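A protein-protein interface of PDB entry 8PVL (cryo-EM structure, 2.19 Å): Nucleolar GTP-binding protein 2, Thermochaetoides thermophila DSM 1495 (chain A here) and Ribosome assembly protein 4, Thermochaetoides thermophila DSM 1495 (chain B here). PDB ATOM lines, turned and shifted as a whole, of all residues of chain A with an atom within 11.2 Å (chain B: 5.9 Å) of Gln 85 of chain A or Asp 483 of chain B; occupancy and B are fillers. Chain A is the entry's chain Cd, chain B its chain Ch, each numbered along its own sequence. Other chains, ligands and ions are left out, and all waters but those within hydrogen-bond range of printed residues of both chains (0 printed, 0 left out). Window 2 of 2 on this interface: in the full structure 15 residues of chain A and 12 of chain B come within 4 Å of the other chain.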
ATOM      1  N   VAL A  82     -27.052   9.535   4.295  1.00  0.00           N
ATOM      2  CA  VAL A  82     -25.681   9.980   4.497  1.00  0.00           C
ATOM      3  C   VAL A  82     -25.636  10.903   5.706  1.00  0.00           C
ATOM      4  O   VAL A  82     -26.645  11.478   6.118  1.00  0.00           O
ATOM      5  CB  VAL A  82     -25.097  10.693   3.256  1.00  0.00           C
ATOM      6  CG1 VAL A  82     -24.912   9.714   2.110  1.00  0.00           C
ATOM      7  CG2 VAL A  82     -25.987  11.848   2.837  1.00  0.00           C
ATOM      8  N   ILE A  83     -24.442  11.037   6.276  1.00  0.00           N
ATOM      9  CA  ILE A  83     -24.231  11.881   7.449  1.00  0.00           C
ATOM     10  C   ILE A  83     -22.800  12.405   7.406  1.00  0.00           C
ATOM     11  O   ILE A  83     -21.888  11.725   6.930  1.00  0.00           O
ATOM     12  CB  ILE A  83     -24.550  11.111   8.755  1.00  0.00           C
ATOM     13  CG1 ILE A  83     -24.550  12.042   9.970  1.00  0.00           C
ATOM     14  CG2 ILE A  83     -23.608   9.926   8.954  1.00  0.00           C
ATOM     15  CD1 ILE A  83     -25.247  11.465  11.179  1.00  0.00           C
ATOM     16  N   SER A  84     -22.612  13.635   7.876  1.00  0.00           N
ATOM     17  CA  SER A  84     -21.312  14.286   7.874  1.00  0.00           C
ATOM     18  C   SER A  84     -20.634  14.161   9.237  1.00  0.00           C
ATOM     19  O   SER A  84     -21.253  13.817  10.249  1.00  0.00           O
ATOM     20  CB  SER A  84     -21.451  15.759   7.481  1.00  0.00           C
ATOM     21  OG  SER A  84     -21.854  16.549   8.583  1.00  0.00           O
ATOM     22  N   GLN A  85     -19.330  14.457   9.245  1.00  0.00           N
ATOM     23  CA  GLN A  85     -18.537  14.341  10.464  1.00  0.00           C
ATOM     24  C   GLN A  85     -18.938  15.374  11.509  1.00  0.00           C
ATOM     25  O   GLN A  85     -18.870  15.091  12.708  1.00  0.00           O
ATOM     26  CB  GLN A  85     -17.049  14.469  10.139  1.00  0.00           C
ATOM     27  CG  GLN A  85     -16.499  13.373   9.237  1.00  0.00           C
ATOM     28  CD  GLN A  85     -16.220  12.075   9.977  1.00  0.00           C
ATOM     29  OE1 GLN A  85     -16.382  11.987  11.194  1.00  0.00           O
ATOM     30  NE2 GLN A  85     -15.790  11.061   9.240  1.00  0.00           N
ATOM     31  N   ASP A  86     -19.353  16.571  11.082  1.00  0.00           N
ATOM     32  CA  ASP A  86     -19.806  17.582  12.035  1.00  0.00           C
ATOM     33  C   ASP A  86     -21.094  17.154  12.728  1.00  0.00           C
ATOM     34  O   ASP A  86     -21.235  17.314  13.949  1.00  0.00           O
ATOM     35  CB  ASP A  86     -20.000  18.918  11.322  1.00  0.00           C
ATOM     36  CG  ASP A  86     -18.899  19.211  10.327  1.00  0.00           C
ATOM     37  OD1 ASP A  86     -18.590  18.323   9.505  1.00  0.00           O
ATOM     38  OD2 ASP A  86     -18.344  20.330  10.362  1.00  0.00           O
ATOM     39  N   THR A  87     -22.041  16.605  11.963  1.00  0.00           N
ATOM     40  CA  THR A  87     -23.272  16.084  12.545  1.00  0.00           C
ATOM     41  C   THR A  87     -22.983  14.909  13.471  1.00  0.00           C
ATOM     42  O   THR A  87     -23.592  14.789  14.543  1.00  0.00           O
ATOM     43  CB  THR A  87     -24.234  15.670  11.431  1.00  0.00           C
ATOM     44  OG1 THR A  87     -24.324  16.724  10.466  1.00  0.00           O
ATOM     45  CG2 THR A  87     -25.611  15.405  11.990  1.00  0.00           C
ATOM     46  N   LEU A  88     -22.038  14.046  13.080  1.00  0.00           N
ATOM     47  CA  LEU A  88     -21.636  12.938  13.942  1.00  0.00           C
ATOM     48  C   LEU A  88     -21.028  13.435  15.249  1.00  0.00           C
ATOM     49  O   LEU A  88     -21.319  12.890  16.317  1.00  0.00           O
ATOM     50  CB  LEU A  88     -20.651  12.030  13.209  1.00  0.00           C
ATOM     51  CG  LEU A  88     -21.262  10.976  12.286  1.00  0.00           C
ATOM     52  CD1 LEU A  88     -20.174  10.228  11.540  1.00  0.00           C
ATOM     53  CD2 LEU A  88     -22.127  10.015  13.079  1.00  0.00           C
ATOM     54  N   GLN A  89     -20.181  14.467  15.183  1.00  0.00           N
ATOM     55  CA  GLN A  89     -19.563  15.012  16.389  1.00  0.00           C
ATOM     56  C   GLN A  89     -20.597  15.655  17.306  1.00  0.00           C
ATOM     57  O   GLN A  89     -20.522  15.508  18.535  1.00  0.00           O
ATOM     58  CB  GLN A  89     -18.482  16.025  16.011  1.00  0.00           C
ATOM     59  CG  GLN A  89     -17.275  16.025  16.938  1.00  0.00           C
ATOM     60  CD  GLN A  89     -16.874  14.631  17.381  1.00  0.00           C
ATOM     61  OE1 GLN A  89     -16.493  13.792  16.565  1.00  0.00           O
ATOM     62  NE2 GLN A  89     -16.961  14.377  18.682  1.00  0.00           N
ATOM     63  N   SER A  90     -21.569  16.366  16.725  1.00  0.00           N
ATOM     64  CA  SER A  90     -22.650  16.940  17.524  1.00  0.00           C
ATOM     65  C   SER A  90     -23.463  15.852  18.215  1.00  0.00           C
ATOM     66  O   SER A  90     -23.801  15.974  19.401  1.00  0.00           O
ATOM     67  CB  SER A  90     -23.553  17.803  16.644  1.00  0.00           C
ATOM     68  OG  SER A  90     -22.819  18.845  16.030  1.00  0.00           O
ATOM     69  N   PHE A  91     -23.764  14.767  17.495  1.00  0.00           N
ATOM     70  CA  PHE A  91     -24.519  13.676  18.100  1.00  0.00           C
ATOM     71  C   PHE A  91     -23.709  12.942  19.163  1.00  0.00           C
ATOM     72  O   PHE A  91     -24.280  12.484  20.155  1.00  0.00           O
ATOM     73  CB  PHE A  91     -25.001  12.708  17.023  1.00  0.00           C
ATOM     74  CG  PHE A  91     -26.218  13.187  16.287  1.00  0.00           C
ATOM     75  CD1 PHE A  91     -27.211  13.888  16.951  1.00  0.00           C
ATOM     76  CD2 PHE A  91     -26.367  12.942  14.934  1.00  0.00           C
ATOM     77  CE1 PHE A  91     -28.332  14.334  16.278  1.00  0.00           C
ATOM     78  CE2 PHE A  91     -27.488  13.383  14.258  1.00  0.00           C
ATOM     79  CZ  PHE A  91     -28.469  14.080  14.929  1.00  0.00           C
ATOM     80  N   ARG A  92     -22.390  12.831  18.984  1.00  0.00           N
ATOM     81  CA  ARG A  92     -21.550  12.210  20.007  1.00  0.00           C
ATOM     82  C   ARG A  92     -21.502  13.054  21.275  1.00  0.00           C
ATOM     83  O   ARG A  92     -21.549  12.514  22.388  1.00  0.00           O
ATOM     84  CB  ARG A  92     -20.140  11.984  19.466  1.00  0.00           C
ATOM     85  CG  ARG A  92     -20.033  10.873  18.444  1.00  0.00           C
ATOM     86  CD  ARG A  92     -18.587  10.538  18.151  1.00  0.00           C
ATOM     87  NE  ARG A  92     -18.456   9.731  16.944  1.00  0.00           N
ATOM     88  CZ  ARG A  92     -17.890  10.152  15.822  1.00  0.00           C
ATOM     89  NH1 ARG A  92     -17.380  11.368  15.718  1.00  0.00           N
ATOM     90  NH2 ARG A  92     -17.834   9.330  14.777  1.00  0.00           N
ATOM     91  N   GLU A  93     -21.405  14.380  21.128  1.00  0.00           N
ATOM     92  CA  GLU A  93     -21.439  15.254  22.298  1.00  0.00           C
ATOM     93  C   GLU A  93     -22.789  15.184  23.006  1.00  0.00           C
ATOM     94  O   GLU A  93     -22.848  15.168  24.243  1.00  0.00           O
ATOM     95  CB  GLU A  93     -21.114  16.689  21.889  1.00  0.00           C
ATOM     96  CG  GLU A  93     -19.671  16.892  21.461  1.00  0.00           C
ATOM     97  CD  GLU A  93     -19.510  18.026  20.469  1.00  0.00           C
ATOM     98  OE1 GLU A  93     -20.536  18.608  20.058  1.00  0.00           O
ATOM     99  OE2 GLU A  93     -18.358  18.333  20.097  1.00  0.00           O
ATOM    100  N   ALA A  94     -23.880  15.126  22.236  1.00  0.00           N
ATOM    101  CA  ALA A  94     -25.205  14.968  22.833  1.00  0.00           C
ATOM    102  C   ALA A  94     -25.341  13.626  23.547  1.00  0.00           C
ATOM    103  O   ALA A  94     -25.967  13.542  24.610  1.00  0.00           O
ATOM    104  CB  ALA A  94     -26.278  15.113  21.757  1.00  0.00           C
ATOM    105  N   PRO A 113     -27.482   6.373  12.711  1.00  0.00           N
ATOM    106  CA  PRO A 113     -26.476   5.293  12.776  1.00  0.00           C
ATOM    107  C   PRO A 113     -25.843   5.223  14.165  1.00  0.00           C
ATOM    108  O   PRO A 113     -24.782   5.775  14.446  1.00  0.00           O
ATOM    109  CB  PRO A 113     -25.476   5.699  11.692  1.00  0.00           C
ATOM    110  CG  PRO A 113     -25.583   7.179  11.618  1.00  0.00           C
ATOM    111  CD  PRO A 113     -27.004   7.532  11.936  1.00  0.00           C
ATOM    112  N   LEU A 116     -22.130   4.410  15.123  1.00  0.00           N
ATOM    113  CA  LEU A 116     -21.136   5.464  14.960  1.00  0.00           C
ATOM    114  C   LEU A 116     -21.280   6.582  15.983  1.00  0.00           C
ATOM    115  O   LEU A 116     -20.448   7.493  16.003  1.00  0.00           O
ATOM    116  CB  LEU A 116     -21.220   6.061  13.551  1.00  0.00           C
ATOM    117  CG  LEU A 116     -21.169   5.118  12.351  1.00  0.00           C
ATOM    118  CD1 LEU A 116     -21.501   5.876  11.078  1.00  0.00           C
ATOM    119  CD2 LEU A 116     -19.807   4.463  12.244  1.00  0.00           C
ATOM    120  N   ILE A 117     -22.311   6.542  16.822  1.00  0.00           N
ATOM    121  CA  ILE A 117     -22.581   7.598  17.784  1.00  0.00           C
ATOM    122  C   ILE A 117     -22.378   7.120  19.217  1.00  0.00           C
ATOM    123  O   ILE A 117     -21.869   7.866  20.057  1.00  0.00           O
ATOM    124  CB  ILE A 117     -24.006   8.161  17.579  1.00  0.00           C
ATOM    125  CG1 ILE A 117     -24.191   8.608  16.129  1.00  0.00           C
ATOM    126  CG2 ILE A 117     -24.279   9.326  18.515  1.00  0.00           C
ATOM    127  CD1 ILE A 117     -25.579   9.098  15.809  1.00  0.00           C
ATOM    128  N   SER B 136      -5.099  20.794   3.265  1.00  0.00           N
ATOM    129  CA  SER B 136      -6.544  20.920   3.183  1.00  0.00           C
ATOM    130  C   SER B 136      -7.136  20.471   1.859  1.00  0.00           C
ATOM    131  O   SER B 136      -8.359  20.315   1.775  1.00  0.00           O
ATOM    132  CB  SER B 136      -6.965  22.375   3.437  1.00  0.00           C
ATOM    133  OG  SER B 136      -6.328  23.255   2.530  1.00  0.00           O
ATOM    134  N   ARG B 443     -11.561  10.078  16.783  1.00  0.00           N
ATOM    135  CA  ARG B 443     -12.655   9.226  16.320  1.00  0.00           C
ATOM    136  C   ARG B 443     -13.314   9.853  15.094  1.00  0.00           C
ATOM    137  O   ARG B 443     -14.291  10.594  15.219  1.00  0.00           O
ATOM    138  CB  ARG B 443     -13.662   9.012  17.445  1.00  0.00           C
ATOM    139  CG  ARG B 443     -14.691   7.939  17.170  1.00  0.00           C
ATOM    140  CD  ARG B 443     -15.804   7.984  18.196  1.00  0.00           C
ATOM    141  NE  ARG B 443     -16.834   6.991  17.915  1.00  0.00           N
ATOM    142  CZ  ARG B 443     -17.906   6.793  18.668  1.00  0.00           C
ATOM    143  NH1 ARG B 443     -18.125   7.508  19.759  1.00  0.00           N
ATOM    144  NH2 ARG B 443     -18.780   5.854  18.318  1.00  0.00           N
ATOM    145  N   GLY B 444     -12.772   9.573  13.913  1.00  0.00           N
ATOM    146  CA  GLY B 444     -13.440   9.975  12.693  1.00  0.00           C
ATOM    147  C   GLY B 444     -13.496   8.906  11.622  1.00  0.00           C
ATOM    148  O   GLY B 444     -14.311   8.993  10.699  1.00  0.00           O
ATOM    149  N   HIS B 445     -12.663   7.879  11.740  1.00  0.00           N
ATOM    150  CA  HIS B 445     -12.595   6.855  10.709  1.00  0.00           C
ATOM    151  C   HIS B 445     -13.631   5.769  10.966  1.00  0.00           C
ATOM    152  O   HIS B 445     -14.016   5.502  12.107  1.00  0.00           O
ATOM    153  CB  HIS B 445     -11.195   6.243  10.641  1.00  0.00           C
ATOM    154  CG  HIS B 445     -10.192   7.099   9.933  1.00  0.00           C
ATOM    155  ND1 HIS B 445     -10.297   7.419   8.596  1.00  0.00           N
ATOM    156  CD2 HIS B 445      -9.061   7.697  10.372  1.00  0.00           C
ATOM    157  CE1 HIS B 445      -9.277   8.179   8.244  1.00  0.00           C
ATOM    158  NE2 HIS B 445      -8.509   8.361   9.304  1.00  0.00           N
ATOM    159  N   VAL B 446     -14.091   5.146   9.882  1.00  0.00           N
ATOM    160  CA  VAL B 446     -15.102   4.098   9.944  1.00  0.00           C
ATOM    161  C   VAL B 446     -14.549   2.740   9.559  1.00  0.00           C
ATOM    162  O   VAL B 446     -15.281   1.744   9.615  1.00  0.00           O
ATOM    163  CB  VAL B 446     -16.321   4.449   9.070  1.00  0.00           C
ATOM    164  CG1 VAL B 446     -17.182   5.484   9.761  1.00  0.00           C
ATOM    165  CG2 VAL B 446     -15.874   4.953   7.712  1.00  0.00           C
ATOM    166  N   THR B 469      -9.828   7.325   2.980  1.00  0.00           N
ATOM    167  CA  THR B 469      -9.677   8.720   3.363  1.00  0.00           C
ATOM    168  C   THR B 469      -8.394   8.946   4.154  1.00  0.00           C
ATOM    169  O   THR B 469      -7.833   8.036   4.792  1.00  0.00           O
ATOM    170  CB  THR B 469     -10.862   9.242   4.203  1.00  0.00           C
ATOM    171  OG1 THR B 469     -10.841   8.642   5.503  1.00  0.00           O
ATOM    172  CG2 THR B 469     -12.202   8.979   3.528  1.00  0.00           C
ATOM    173  N   LEU B 470      -7.948  10.203   4.097  1.00  0.00           N
ATOM    174  CA  LEU B 470      -6.959  10.751   5.006  1.00  0.00           C
ATOM    175  C   LEU B 470      -7.645  11.736   5.942  1.00  0.00           C
ATOM    176  O   LEU B 470      -8.621  12.394   5.573  1.00  0.00           O
ATOM    177  CB  LEU B 470      -5.834  11.476   4.260  1.00  0.00           C
ATOM    178  CG  LEU B 470      -5.025  10.818   3.144  1.00  0.00           C
ATOM    179  CD1 LEU B 470      -3.734  11.592   2.946  1.00  0.00           C
ATOM    180  CD2 LEU B 470      -4.737   9.367   3.426  1.00  0.00           C
ATOM    181  N   LYS B 471      -7.136  11.829   7.162  1.00  0.00           N
ATOM    182  CA  LYS B 471      -7.666  12.784   8.127  1.00  0.00           C
ATOM    183  C   LYS B 471      -6.521  13.463   8.853  1.00  0.00           C
ATOM    184  O   LYS B 471      -5.639  12.792   9.391  1.00  0.00           O
ATOM    185  CB  LYS B 471      -8.605  12.102   9.128  1.00  0.00           C
ATOM    186  CG  LYS B 471      -9.917  11.656   8.517  1.00  0.00           C
ATOM    187  CD  LYS B 471     -10.967  11.365   9.556  1.00  0.00           C
ATOM    188  CE  LYS B 471     -12.130  10.637   8.921  1.00  0.00           C
ATOM    189  NZ  LYS B 471     -12.528  11.248   7.630  1.00  0.00           N
ATOM    190  N   VAL B 472      -6.536  14.791   8.862  1.00  0.00           N
ATOM    191  CA  VAL B 472      -5.569  15.589   9.600  1.00  0.00           C
ATOM    192  C   VAL B 472      -6.207  15.986  10.919  1.00  0.00           C
ATOM    193  O   VAL B 472      -7.293  16.581  10.939  1.00  0.00           O
ATOM    194  CB  VAL B 472      -5.139  16.831   8.801  1.00  0.00           C
ATOM    195  CG1 VAL B 472      -4.107  17.629   9.583  1.00  0.00           C
ATOM    196  CG2 VAL B 472      -4.595  16.426   7.446  1.00  0.00           C
ATOM    197  N   LEU B 480     -10.711  17.012  14.584  1.00  0.00           N
ATOM    198  CA  LEU B 480     -10.489  16.777  13.162  1.00  0.00           C
ATOM    199  C   LEU B 480     -10.302  18.120  12.472  1.00  0.00           C
ATOM    200  O   LEU B 480     -11.267  18.843  12.221  1.00  0.00           O
ATOM    201  CB  LEU B 480     -11.661  16.009  12.563  1.00  0.00           C
ATOM    202  CG  LEU B 480     -11.596  15.729  11.062  1.00  0.00           C
ATOM    203  CD1 LEU B 480     -10.387  14.882  10.744  1.00  0.00           C
ATOM    204  CD2 LEU B 480     -12.866  15.051  10.584  1.00  0.00           C
ATOM    205  N   ALA B 481      -9.048  18.471  12.184  1.00  0.00           N
ATOM    206  CA  ALA B 481      -8.781  19.713  11.473  1.00  0.00           C
ATOM    207  C   ALA B 481      -9.221  19.616  10.019  1.00  0.00           C
ATOM    208  O   ALA B 481      -9.971  20.468   9.532  1.00  0.00           O
ATOM    209  CB  ALA B 481      -7.295  20.060  11.567  1.00  0.00           C
ATOM    210  N   MET B 482      -8.771  18.582   9.304  1.00  0.00           N
ATOM    211  CA  MET B 482      -9.056  18.490   7.877  1.00  0.00           C
ATOM    212  C   MET B 482      -9.478  17.080   7.495  1.00  0.00           C
ATOM    213  O   MET B 482      -8.945  16.099   8.015  1.00  0.00           O
ATOM    214  CB  MET B 482      -7.842  18.904   7.032  1.00  0.00           C
ATOM    215  CG  MET B 482      -7.426  20.357   7.196  1.00  0.00           C
ATOM    216  SD  MET B 482      -8.658  21.506   6.562  1.00  0.00           S
ATOM    217  CE  MET B 482      -7.905  23.074   6.980  1.00  0.00           C
ATOM    218  N   ASP B 483     -10.430  16.991   6.573  1.00  0.00           N
ATOM    219  CA  ASP B 483     -10.838  15.733   5.962  1.00  0.00           C
ATOM    220  C   ASP B 483     -10.366  15.721   4.516  1.00  0.00           C
ATOM    221  O   ASP B 483     -10.612  16.679   3.777  1.00  0.00           O
ATOM    222  CB  ASP B 483     -12.355  15.560   6.029  1.00  0.00           C
ATOM    223  CG  ASP B 483     -12.775  14.110   6.110  1.00  0.00           C
ATOM    224  OD1 ASP B 483     -11.993  13.237   5.684  1.00  0.00           O
ATOM    225  OD2 ASP B 483     -13.893  13.843   6.595  1.00  0.00           O
ATOM    226  N   LEU B 484      -9.689  14.645   4.109  1.00  0.00           N
ATOM    227  CA  LEU B 484      -9.116  14.524   2.771  1.00  0.00           C
ATOM    228  C   LEU B 484      -9.718  13.301   2.094  1.00  0.00           C
ATOM    229  O   LEU B 484      -9.227  12.171   2.269  1.00  0.00           O
ATOM    230  CB  LEU B 484      -7.594  14.426   2.836  1.00  0.00           C
ATOM    231  CG  LEU B 484      -6.880  15.515   3.638  1.00  0.00           C
ATOM    232  CD1 LEU B 484      -5.382  15.268   3.666  1.00  0.00           C
ATOM    233  CD2 LEU B 484      -7.188  16.893   3.080  1.00  0.00           C
ATOM    234  N   PRO B 485     -10.814  13.470   1.359  1.00  0.00           N
ATOM    235  CA  PRO B 485     -11.312  12.406   0.488  1.00  0.00           C
ATOM    236  C   PRO B 485     -10.747  12.541  -0.919  1.00  0.00           C
ATOM    237  O   PRO B 485     -10.176  13.564  -1.299  1.00  0.00           O
ATOM    238  CB  PRO B 485     -12.834  12.637   0.485  1.00  0.00           C
ATOM    239  CG  PRO B 485     -13.075  13.844   1.388  1.00  0.00           C
ATOM    240  CD  PRO B 485     -11.782  14.570   1.457  1.00  0.00           C
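The side-chain amide nitrogen (NE2) of Gln 85 of chain A sits at hydrogen-bond distance from the backbone carbonyl oxygen (O) of Gly 444 of chain B, 2.9 Å away.
The guanidinium group (NH1) of Arg 92 of chain A lies within hydrogen-bond range of the backbone carbonyl oxygen (O) of Arg 443 of chain B, at 3.2 Å.
The guanidinium group of Arg 443 of chain B lies within hydrogen-bond range of the backbone carbonyl oxygen of Leu 116 of chain A (3.3 Å).
Hydrophobic or aromatic side chains of chain B within 4 Å of the printed part of chain A: Val 446.
Along chain B the printed residues that touch a printed residue of chain A span positions 443 to 483.
Of the 16 printed residues of chain A, 4 touch a printed residue of chain B.
Hydrophobic or aromatic side chains of chain A within 4 Å of the printed part of chain B: Leu 116.
Among the printed residues, 7 pairs touch across the chains.
Among the printed residues, no Asp or Glu carboxylate lies within 4 Å of a Lys or Arg side-chain nitrogen of the other chain.
Among the printed residues, merely in contact across the chains: Gln 85 of chain A with Lys 471 of chain B, Gln 85 of chain A with Asp 483 of chain B, Leu 116 of chain A with Val 446 of chain B and Ile 117 of chain A with Arg 443 of chain B.
OE1 of Gln 89 of chain A sits at hydrogen-bond distance from NH1 of Arg 92 of chain A (2.7 Å).
The side-chain carboxylate (OD1) of Asp 483 of chain B is in salt-bridge range of the side-chain amino group (NZ) of Lys 471 of chain B, at 2.8 Å.
O of Leu 116 of chain A lies within hydrogen-bond range of NE of Arg 92 of chain A (3.1 Å).
Ser 84 of chain A touches none of the printed residues of chain B.
Of chain B, only Gly 444 (2.9 Å), Lys 471 (3.6 Å) and Asp 483 (3.7 Å) come within 4 Å of Gln 85 of chain A.
Asp 86 of chain A touches none of the printed residues of chain B.
Printed residues of chain B within 4 Å of Arg 92 of chain A: Arg 443.
Of the printed residues of chain B, Leu 116 of chain A touches Arg 443 and Val 446.
Of the printed residues of chain B, Ile 117 of chain A touches Arg 443.
Of the printed residues of chain A, Arg 443 of chain B touches Arg 92, Leu 116 and Ile 117.
Printed residues of chain A within 4 Å of Val 446 of chain B: Leu 116 (3.8 Å).
No residue of chain A comes within 4 Å of Thr 469 of chain B.
Printed residues of chain A within 4 Å of Lys 471 of chain B: Gln 85 (3.6 Å).
No residue of chain A comes within 4 Å of Ala 481 of chain B.
Printed residues of chain A within 4 Å of Asp 483 of chain B: Gln 85.
Pro 485 of chain B touches none of the printed residues of chain A.
The nearest residue of chain A that does not touch Asp 483 of chain B is Asp 86 of chain A (7.1 Å).
The nearest printed residue of chain B that does not touch Arg 92 of chain A is Gly 444 of chain B (4.9 Å).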
